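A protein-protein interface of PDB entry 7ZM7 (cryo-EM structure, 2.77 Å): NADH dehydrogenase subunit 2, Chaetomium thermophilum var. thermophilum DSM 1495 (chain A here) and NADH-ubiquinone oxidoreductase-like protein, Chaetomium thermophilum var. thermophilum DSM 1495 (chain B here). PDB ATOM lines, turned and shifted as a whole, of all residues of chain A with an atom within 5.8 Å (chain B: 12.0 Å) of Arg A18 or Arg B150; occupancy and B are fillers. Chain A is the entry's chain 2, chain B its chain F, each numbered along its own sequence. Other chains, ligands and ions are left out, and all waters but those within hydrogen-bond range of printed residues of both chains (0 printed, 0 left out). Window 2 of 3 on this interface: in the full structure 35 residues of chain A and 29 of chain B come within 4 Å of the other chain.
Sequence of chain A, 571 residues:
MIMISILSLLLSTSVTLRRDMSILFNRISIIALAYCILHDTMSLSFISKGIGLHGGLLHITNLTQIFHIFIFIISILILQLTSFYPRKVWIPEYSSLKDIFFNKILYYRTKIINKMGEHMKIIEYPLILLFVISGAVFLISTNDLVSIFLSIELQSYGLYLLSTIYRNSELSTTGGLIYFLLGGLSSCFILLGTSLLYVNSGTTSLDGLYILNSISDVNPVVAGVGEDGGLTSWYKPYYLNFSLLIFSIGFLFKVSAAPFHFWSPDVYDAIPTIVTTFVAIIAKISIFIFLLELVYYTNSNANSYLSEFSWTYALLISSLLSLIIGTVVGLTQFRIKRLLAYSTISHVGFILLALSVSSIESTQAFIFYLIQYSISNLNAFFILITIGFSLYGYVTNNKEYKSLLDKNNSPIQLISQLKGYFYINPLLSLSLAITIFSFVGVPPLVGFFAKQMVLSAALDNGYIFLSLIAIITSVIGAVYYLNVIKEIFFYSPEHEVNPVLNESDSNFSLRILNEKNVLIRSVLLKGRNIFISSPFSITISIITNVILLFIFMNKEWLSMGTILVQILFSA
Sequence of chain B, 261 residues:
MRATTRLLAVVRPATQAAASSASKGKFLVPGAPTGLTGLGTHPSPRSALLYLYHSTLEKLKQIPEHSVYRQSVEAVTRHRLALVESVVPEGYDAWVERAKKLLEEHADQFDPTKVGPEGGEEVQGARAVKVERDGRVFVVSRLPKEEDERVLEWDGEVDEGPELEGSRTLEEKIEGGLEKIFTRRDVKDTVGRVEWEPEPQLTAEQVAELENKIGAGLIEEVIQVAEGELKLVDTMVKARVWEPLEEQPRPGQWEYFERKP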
ATOM      1  N   THR A  16      -4.440   2.238  26.489  1.00  0.00           N
ATOM      2  CA  THR A  16      -4.977   0.888  26.466  1.00  0.00           C
ATOM      3  C   THR A  16      -6.448   0.914  26.835  1.00  0.00           C
ATOM      4  O   THR A  16      -6.912   1.809  27.540  1.00  0.00           O
ATOM      5  CB  THR A  16      -4.228  -0.052  27.423  1.00  0.00           C
ATOM      6  OG1 THR A  16      -4.559  -1.407  27.108  1.00  0.00           O
ATOM      7  CG2 THR A  16      -4.612   0.215  28.859  1.00  0.00           C
ATOM      8  N   LEU A  17      -7.182  -0.082  26.332  1.00  0.00           N
ATOM      9  CA  LEU A  17      -8.610  -0.238  26.702  1.00  0.00           C
ATOM     10  C   LEU A  17      -8.792  -1.676  27.192  1.00  0.00           C
ATOM     11  O   LEU A  17      -9.937  -2.055  27.476  1.00  0.00           O
ATOM     12  CB  LEU A  17      -9.467   0.027  25.462  1.00  0.00           C
ATOM     13  CG  LEU A  17     -10.320   1.295  25.497  1.00  0.00           C
ATOM     14  CD1 LEU A  17      -9.453   2.540  25.430  1.00  0.00           C
ATOM     15  CD2 LEU A  17     -11.318   1.299  24.354  1.00  0.00           C
ATOM     16  N   ARG A  18      -7.703  -2.443  27.285  1.00  0.00           N
ATOM     17  CA  ARG A  18      -7.800  -3.881  27.651  1.00  0.00           C
ATOM     18  C   ARG A  18      -8.032  -4.038  29.156  1.00  0.00           C
ATOM     19  O   ARG A  18      -7.230  -3.499  29.933  1.00  0.00           O
ATOM     20  CB  ARG A  18      -6.532  -4.611  27.202  1.00  0.00           C
ATOM     21  CG  ARG A  18      -6.440  -4.844  25.701  1.00  0.00           C
ATOM     22  CD  ARG A  18      -5.057  -5.313  25.291  1.00  0.00           C
ATOM     23  NE  ARG A  18      -4.660  -6.543  25.959  1.00  0.00           N
ATOM     24  CZ  ARG A  18      -3.483  -7.140  25.806  1.00  0.00           C
ATOM     25  NH1 ARG A  18      -2.575  -6.614  25.003  1.00  0.00           N
ATOM     26  NH2 ARG A  18      -3.218  -8.258  26.455  1.00  0.00           N
ATOM     27  N   ARG A  19      -9.073  -4.784  29.539  1.00  0.00           N
ATOM     28  CA  ARG A  19      -9.410  -4.951  30.975  1.00  0.00           C
ATOM     29  C   ARG A  19      -8.580  -6.087  31.570  1.00  0.00           C
ATOM     30  O   ARG A  19      -8.422  -6.070  32.795  1.00  0.00           O
ATOM     31  CB  ARG A  19     -10.913  -5.176  31.166  1.00  0.00           C
ATOM     32  CG  ARG A  19     -11.771  -3.968  30.827  1.00  0.00           C
ATOM     33  CD  ARG A  19     -13.229  -4.241  31.128  1.00  0.00           C
ATOM     34  NE  ARG A  19     -13.621  -5.552  30.634  1.00  0.00           N
ATOM     35  CZ  ARG A  19     -14.249  -5.779  29.487  1.00  0.00           C
ATOM     36  NH1 ARG A  19     -14.577  -4.771  28.698  1.00  0.00           N
ATOM     37  NH2 ARG A  19     -14.547  -7.016  29.135  1.00  0.00           N
ATOM     38  N   ASP A  20      -8.099  -7.052  30.790  1.00  0.00           N
ATOM     39  CA  ASP A  20      -7.207  -8.091  31.282  1.00  0.00           C
ATOM     40  C   ASP A  20      -5.895  -7.519  31.776  1.00  0.00           C
ATOM     41  O   ASP A  20      -5.166  -8.190  32.503  1.00  0.00           O
ATOM     42  CB  ASP A  20      -6.972  -9.127  30.177  1.00  0.00           C
ATOM     43  CG  ASP A  20      -6.185  -8.580  29.010  1.00  0.00           C
ATOM     44  OD1 ASP A  20      -6.697  -7.730  28.273  1.00  0.00           O
ATOM     45  OD2 ASP A  20      -5.069  -9.037  28.768  1.00  0.00           O
ATOM     46  N   MET A  21      -5.699  -6.215  31.616  1.00  0.00           N
ATOM     47  CA  MET A  21      -4.383  -5.553  31.773  1.00  0.00           C
ATOM     48  C   MET A  21      -4.439  -4.776  33.088  1.00  0.00           C
ATOM     49  O   MET A  21      -3.564  -3.938  33.334  1.00  0.00           O
ATOM     50  CB  MET A  21      -4.183  -4.615  30.575  1.00  0.00           C
ATOM     51  CG  MET A  21      -2.821  -3.964  30.458  1.00  0.00           C
ATOM     52  SD  MET A  21      -1.452  -5.112  30.668  1.00  0.00           S
ATOM     53  CE  MET A  21      -0.198  -3.988  31.278  1.00  0.00           C
ATOM     54  N   SER A  22      -5.422  -5.085  33.938  1.00  0.00           N
ATOM     55  CA  SER A  22      -5.617  -4.354  35.217  1.00  0.00           C
ATOM     56  C   SER A  22      -4.807  -5.001  36.337  1.00  0.00           C
ATOM     57  O   SER A  22      -4.216  -4.263  37.129  1.00  0.00           O
ATOM     58  CB  SER A  22      -7.068  -4.331  35.572  1.00  0.00           C
ATOM     59  OG  SER A  22      -7.648  -5.595  35.321  1.00  0.00           O
ATOM     60  N   LYS A 121     -11.248  -6.055  36.843  1.00  0.00           N
ATOM     61  CA  LYS A 121     -11.492  -5.493  35.483  1.00  0.00           C
ATOM     62  C   LYS A 121     -11.341  -3.970  35.417  1.00  0.00           C
ATOM     63  O   LYS A 121     -10.894  -3.494  34.361  1.00  0.00           O
ATOM     64  CB  LYS A 121     -12.831  -5.981  34.922  1.00  0.00           C
ATOM     65  CG  LYS A 121     -12.846  -7.453  34.536  1.00  0.00           C
ATOM     66  CD  LYS A 121     -14.186  -7.944  34.062  1.00  0.00           C
ATOM     67  CE  LYS A 121     -14.249  -8.150  32.565  1.00  0.00           C
ATOM     68  NZ  LYS A 121     -15.623  -8.464  32.113  1.00  0.00           N
ATOM     69  N   ILE A 123      -9.620  -0.576  35.218  1.00  0.00           N
ATOM     70  CA  ILE A 123      -8.177  -0.398  34.871  1.00  0.00           C
ATOM     71  C   ILE A 123      -7.654   0.828  35.608  1.00  0.00           C
ATOM     72  O   ILE A 123      -6.439   0.914  35.842  1.00  0.00           O
ATOM     73  CB  ILE A 123      -7.968  -0.267  33.349  1.00  0.00           C
ATOM     74  CG1 ILE A 123      -8.870  -1.243  32.613  1.00  0.00           C
ATOM     75  CG2 ILE A 123      -6.525  -0.566  32.998  1.00  0.00           C
ATOM     76  CD1 ILE A 123      -8.366  -2.625  32.817  1.00  0.00           C
ATOM     77  N   LYS B 145     -10.766 -15.982  15.124  1.00  0.00           N
ATOM     78  CA  LYS B 145     -10.622 -14.769  14.334  1.00  0.00           C
ATOM     79  C   LYS B 145      -9.333 -14.040  14.689  1.00  0.00           C
ATOM     80  O   LYS B 145      -8.973 -13.921  15.863  1.00  0.00           O
ATOM     81  CB  LYS B 145     -11.822 -13.852  14.554  1.00  0.00           C
ATOM     82  CG  LYS B 145     -13.157 -14.511  14.260  1.00  0.00           C
ATOM     83  CD  LYS B 145     -14.316 -13.607  14.637  1.00  0.00           C
ATOM     84  CE  LYS B 145     -14.337 -13.338  16.131  1.00  0.00           C
ATOM     85  NZ  LYS B 145     -14.426 -14.603  16.912  1.00  0.00           N
ATOM     86  N   GLU B 146      -8.638 -13.551  13.667  1.00  0.00           N
ATOM     87  CA  GLU B 146      -7.405 -12.795  13.859  1.00  0.00           C
ATOM     88  C   GLU B 146      -7.775 -11.366  14.227  1.00  0.00           C
ATOM     89  O   GLU B 146      -8.344 -10.635  13.412  1.00  0.00           O
ATOM     90  CB  GLU B 146      -6.539 -12.820  12.603  1.00  0.00           C
ATOM     91  CG  GLU B 146      -6.162 -14.203  12.123  1.00  0.00           C
ATOM     92  CD  GLU B 146      -7.210 -14.794  11.210  1.00  0.00           C
ATOM     93  OE1 GLU B 146      -8.049 -14.024  10.700  1.00  0.00           O
ATOM     94  OE2 GLU B 146      -7.192 -16.024  10.997  1.00  0.00           O
ATOM     95  N   GLU B 147      -7.450 -10.966  15.449  1.00  0.00           N
ATOM     96  CA  GLU B 147      -7.731  -9.624  15.927  1.00  0.00           C
ATOM     97  C   GLU B 147      -6.441  -8.958  16.377  1.00  0.00           C
ATOM     98  O   GLU B 147      -5.433  -9.619  16.637  1.00  0.00           O
ATOM     99  CB  GLU B 147      -8.742  -9.641  17.077  1.00  0.00           C
ATOM    100  CG  GLU B 147     -10.003 -10.413  16.761  1.00  0.00           C
ATOM    101  CD  GLU B 147     -10.644  -9.958  15.469  1.00  0.00           C
ATOM    102  OE1 GLU B 147     -10.884  -8.742  15.320  1.00  0.00           O
ATOM    103  OE2 GLU B 147     -10.906 -10.815  14.601  1.00  0.00           O
ATOM    104  N   ASP B 148      -6.483  -7.633  16.452  1.00  0.00           N
ATOM    105  CA  ASP B 148      -5.332  -6.889  16.933  1.00  0.00           C
ATOM    106  C   ASP B 148      -5.049  -7.238  18.385  1.00  0.00           C
ATOM    107  O   ASP B 148      -5.959  -7.316  19.213  1.00  0.00           O
ATOM    108  CB  ASP B 148      -5.570  -5.385  16.801  1.00  0.00           C
ATOM    109  CG  ASP B 148      -4.333  -4.568  17.125  1.00  0.00           C
ATOM    110  OD1 ASP B 148      -3.257  -5.161  17.319  1.00  0.00           O
ATOM    111  OD2 ASP B 148      -4.446  -3.332  17.207  1.00  0.00           O
ATOM    112  N   GLU B 149      -3.769  -7.432  18.693  1.00  0.00           N
ATOM    113  CA  GLU B 149      -3.365  -7.664  20.068  1.00  0.00           C
ATOM    114  C   GLU B 149      -3.692  -6.487  20.969  1.00  0.00           C
ATOM    115  O   GLU B 149      -3.905  -6.688  22.167  1.00  0.00           O
ATOM    116  CB  GLU B 149      -1.868  -7.952  20.125  1.00  0.00           C
ATOM    117  CG  GLU B 149      -1.472  -9.257  19.466  1.00  0.00           C
ATOM    118  CD  GLU B 149      -1.324  -9.121  17.965  1.00  0.00           C
ATOM    119  OE1 GLU B 149      -1.471  -7.989  17.455  1.00  0.00           O
ATOM    120  OE2 GLU B 149      -1.068 -10.143  17.295  1.00  0.00           O
ATOM    121  N   ARG B 150      -3.743  -5.274  20.429  1.00  0.00           N
ATOM    122  CA  ARG B 150      -4.011  -4.086  21.222  1.00  0.00           C
ATOM    123  C   ARG B 150      -5.459  -3.986  21.658  1.00  0.00           C
ATOM    124  O   ARG B 150      -5.781  -3.118  22.469  1.00  0.00           O
ATOM    125  CB  ARG B 150      -3.619  -2.816  20.456  1.00  0.00           C
ATOM    126  CG  ARG B 150      -2.125  -2.513  20.434  1.00  0.00           C
ATOM    127  CD  ARG B 150      -1.390  -3.211  19.322  1.00  0.00           C
ATOM    128  NE  ARG B 150      -1.893  -2.798  18.014  1.00  0.00           N
ATOM    129  CZ  ARG B 150      -1.475  -1.724  17.348  1.00  0.00           C
ATOM    130  NH1 ARG B 150      -2.000  -1.437  16.172  1.00  0.00           N
ATOM    131  NH2 ARG B 150      -0.527  -0.946  17.848  1.00  0.00           N
ATOM    132  N   VAL B 151      -6.341  -4.841  21.153  1.00  0.00           N
ATOM    133  CA  VAL B 151      -7.751  -4.790  21.517  1.00  0.00           C
ATOM    134  C   VAL B 151      -8.255  -6.099  22.106  1.00  0.00           C
ATOM    135  O   VAL B 151      -9.390  -6.144  22.596  1.00  0.00           O
ATOM    136  CB  VAL B 151      -8.621  -4.369  20.309  1.00  0.00           C
ATOM    137  CG1 VAL B 151      -8.665  -5.465  19.257  1.00  0.00           C
ATOM    138  CG2 VAL B 151     -10.019  -3.912  20.735  1.00  0.00           C
ATOM    139  N   LEU B 152      -7.442  -7.144  22.137  1.00  0.00           N
ATOM    140  CA  LEU B 152      -7.901  -8.471  22.523  1.00  0.00           C
ATOM    141  C   LEU B 152      -7.681  -8.689  24.019  1.00  0.00           C
ATOM    142  O   LEU B 152      -6.541  -8.670  24.489  1.00  0.00           O
ATOM    143  CB  LEU B 152      -7.157  -9.513  21.694  1.00  0.00           C
ATOM    144  CG  LEU B 152      -7.756 -10.897  21.551  1.00  0.00           C
ATOM    145  CD1 LEU B 152      -9.074 -10.761  20.856  1.00  0.00           C
ATOM    146  CD2 LEU B 152      -6.839 -11.735  20.724  1.00  0.00           C
ATOM    147  N   GLU B 153      -8.767  -8.905  24.762  1.00  0.00           N
ATOM    148  CA  GLU B 153      -8.714  -9.174  26.195  1.00  0.00           C
ATOM    149  C   GLU B 153      -8.694 -10.672  26.452  1.00  0.00           C
ATOM    150  O   GLU B 153      -9.588 -11.393  25.998  1.00  0.00           O
ATOM    151  CB  GLU B 153      -9.915  -8.580  26.923  1.00  0.00           C
ATOM    152  CG  GLU B 153      -9.883  -7.092  27.156  1.00  0.00           C
ATOM    153  CD  GLU B 153     -11.270  -6.536  27.339  1.00  0.00           C
ATOM    154  OE1 GLU B 153     -12.225  -7.247  26.985  1.00  0.00           O
ATOM    155  OE2 GLU B 153     -11.415  -5.406  27.837  1.00  0.00           O
ATOM    156  N   TRP B 154      -7.700 -11.127  27.212  1.00  0.00           N
ATOM    157  CA  TRP B 154      -7.591 -12.524  27.638  1.00  0.00           C
ATOM    158  C   TRP B 154      -7.512 -13.471  26.449  1.00  0.00           C
ATOM    159  O   TRP B 154      -8.077 -14.560  26.468  1.00  0.00           O
ATOM    160  CB  TRP B 154      -8.747 -12.924  28.554  1.00  0.00           C
ATOM    161  CG  TRP B 154      -8.701 -12.318  29.903  1.00  0.00           C
ATOM    162  CD1 TRP B 154      -7.821 -12.602  30.890  1.00  0.00           C
ATOM    163  CD2 TRP B 154      -9.590 -11.336  30.427  1.00  0.00           C
ATOM    164  NE1 TRP B 154      -8.098 -11.853  31.995  1.00  0.00           N
ATOM    165  CE2 TRP B 154      -9.184 -11.065  31.737  1.00  0.00           C
ATOM    166  CE3 TRP B 154     -10.685 -10.644  29.905  1.00  0.00           C
ATOM    167  CZ2 TRP B 154      -9.831 -10.144  32.537  1.00  0.00           C
ATOM    168  CZ3 TRP B 154     -11.318  -9.721  30.693  1.00  0.00           C
ATOM    169  CH2 TRP B 154     -10.893  -9.481  31.998  1.00  0.00           C
ATOM    170  N   ASP B 155      -6.812 -13.042  25.404  1.00  0.00           N
ATOM    171  CA  ASP B 155      -6.644 -13.828  24.187  1.00  0.00           C
ATOM    172  C   ASP B 155      -7.978 -14.151  23.538  1.00  0.00           C
ATOM    173  O   ASP B 155      -8.097 -15.113  22.785  1.00  0.00           O
ATOM    174  CB  ASP B 155      -5.856 -15.114  24.456  1.00  0.00           C
ATOM    175  CG  ASP B 155      -4.365 -14.880  24.514  1.00  0.00           C
ATOM    176  OD1 ASP B 155      -3.928 -13.759  24.193  1.00  0.00           O
ATOM    177  OD2 ASP B 155      -3.628 -15.819  24.875  1.00  0.00           O
ATOM    178  N   GLY B 156      -8.988 -13.350  23.822  1.00  0.00           N
ATOM    179  CA  GLY B 156     -10.289 -13.555  23.240  1.00  0.00           C
ATOM    180  C   GLY B 156     -11.194 -14.523  23.957  1.00  0.00           C
ATOM    181  O   GLY B 156     -12.262 -14.835  23.428  1.00  0.00           O
ATOM    182  N   GLU B 157     -10.823 -15.003  25.136  1.00  0.00           N
ATOM    183  CA  GLU B 157     -11.699 -15.911  25.859  1.00  0.00           C
ATOM    184  C   GLU B 157     -13.017 -15.231  26.172  1.00  0.00           C
ATOM    185  O   GLU B 157     -13.041 -14.151  26.766  1.00  0.00           O
ATOM    186  CB  GLU B 157     -11.056 -16.396  27.153  1.00  0.00           C
ATOM    187  CG  GLU B 157     -12.014 -17.280  27.937  1.00  0.00           C
ATOM    188  CD  GLU B 157     -11.376 -18.091  29.030  1.00  0.00           C
ATOM    189  OE1 GLU B 157     -10.147 -18.061  29.174  1.00  0.00           O
ATOM    190  OE2 GLU B 157     -12.125 -18.762  29.754  1.00  0.00           O
ATOM    191  N   ASP B 159     -16.268 -13.862  27.719  1.00  0.00           N
ATOM    192  CA  ASP B 159     -16.595 -13.470  29.085  1.00  0.00           C
ATOM    193  C   ASP B 159     -18.049 -13.828  29.356  1.00  0.00           C
ATOM    194  O   ASP B 159     -18.964 -13.160  28.876  1.00  0.00           O
ATOM    195  CB  ASP B 159     -16.339 -11.984  29.293  1.00  0.00           C
ATOM    196  CG  ASP B 159     -16.895 -11.472  30.609  1.00  0.00           C
ATOM    197  OD1 ASP B 159     -16.863 -12.216  31.609  1.00  0.00           O
ATOM    198  OD2 ASP B 159     -17.372 -10.319  30.637  1.00  0.00           O
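The side-chain carboxylate (OD2) of Asp B148 is in salt-bridge range of the guanidinium group (NE) of Arg B150 (2.7 Å).
OG1 of Thr A16 lies within hydrogen-bond range of N of Arg A18, 3.3 Å away.
NH2 of Arg A18 is in salt-bridge range of OD2 of Asp A20, 3.1 Å away.
The backbone carbonyl oxygen of Arg A19 lies within hydrogen-bond range of the side-chain hydroxyl of Ser A22, at 2.7 Å.
Leu A17 touches just one residue of chain B: Glu B153.
Arg A18 touches just these residues of chain B: Glu B149 (3.1 Å), Arg B150 (3.6 Å), Leu B152 (3.2 Å) and Glu B153 (3.9 Å).
Of chain B, only Leu B152, Glu B153 and Trp B154 come within 4 Å of Asp A20.
No residue of chain B comes within 4 Å of Met A21.
Ser A22 touches none of the printed residues of chain B.
Arg B150 touches just one residue of chain A: Arg A18.
Of the printed residues of chain A, Leu B152 touches Arg A18 and Asp A20.
Of the printed residues of chain A, Asp B159 touches Lys A121.
The nearest residue of chain B that does not touch Arg A18 is Val B151 (4.2 Å).
The nearest printed residue of chain B that does not touch Lys A121 is Glu B153 (6.0 Å).
Among the printed residues, Asp or Glu carboxylates within 4 Å of a Lys or Arg side-chain nitrogen of the other chain: Arg A19 with Glu B153 (3.2 Å) and Lys A121 with Asp B159 (2.9 Å).
O of Glu B149 is in hydrogen-bond range of NH1 of Arg A18 (3.1 Å).
The backbone carbonyl oxygen (O) of Leu B152 is in hydrogen-bond range of the guanidinium group (NE) of Arg A18.
The side-chain carboxylate of Glu B153 lies within salt-bridge range of the guanidinium group of Arg A19 (3.2 Å).
OD2 of Asp B159 is in salt-bridge range of NZ of Lys A121 (2.9 Å).
Among the printed residues, pairs that only touch across the chains: Asp A20 with Glu B153, Asp A20 with Trp B154, Arg A18 with Arg B150, Lys A121 with Trp B154, Leu A17 with Glu B153, Arg A18 with Glu B153 and Asp A20 with Leu B152.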
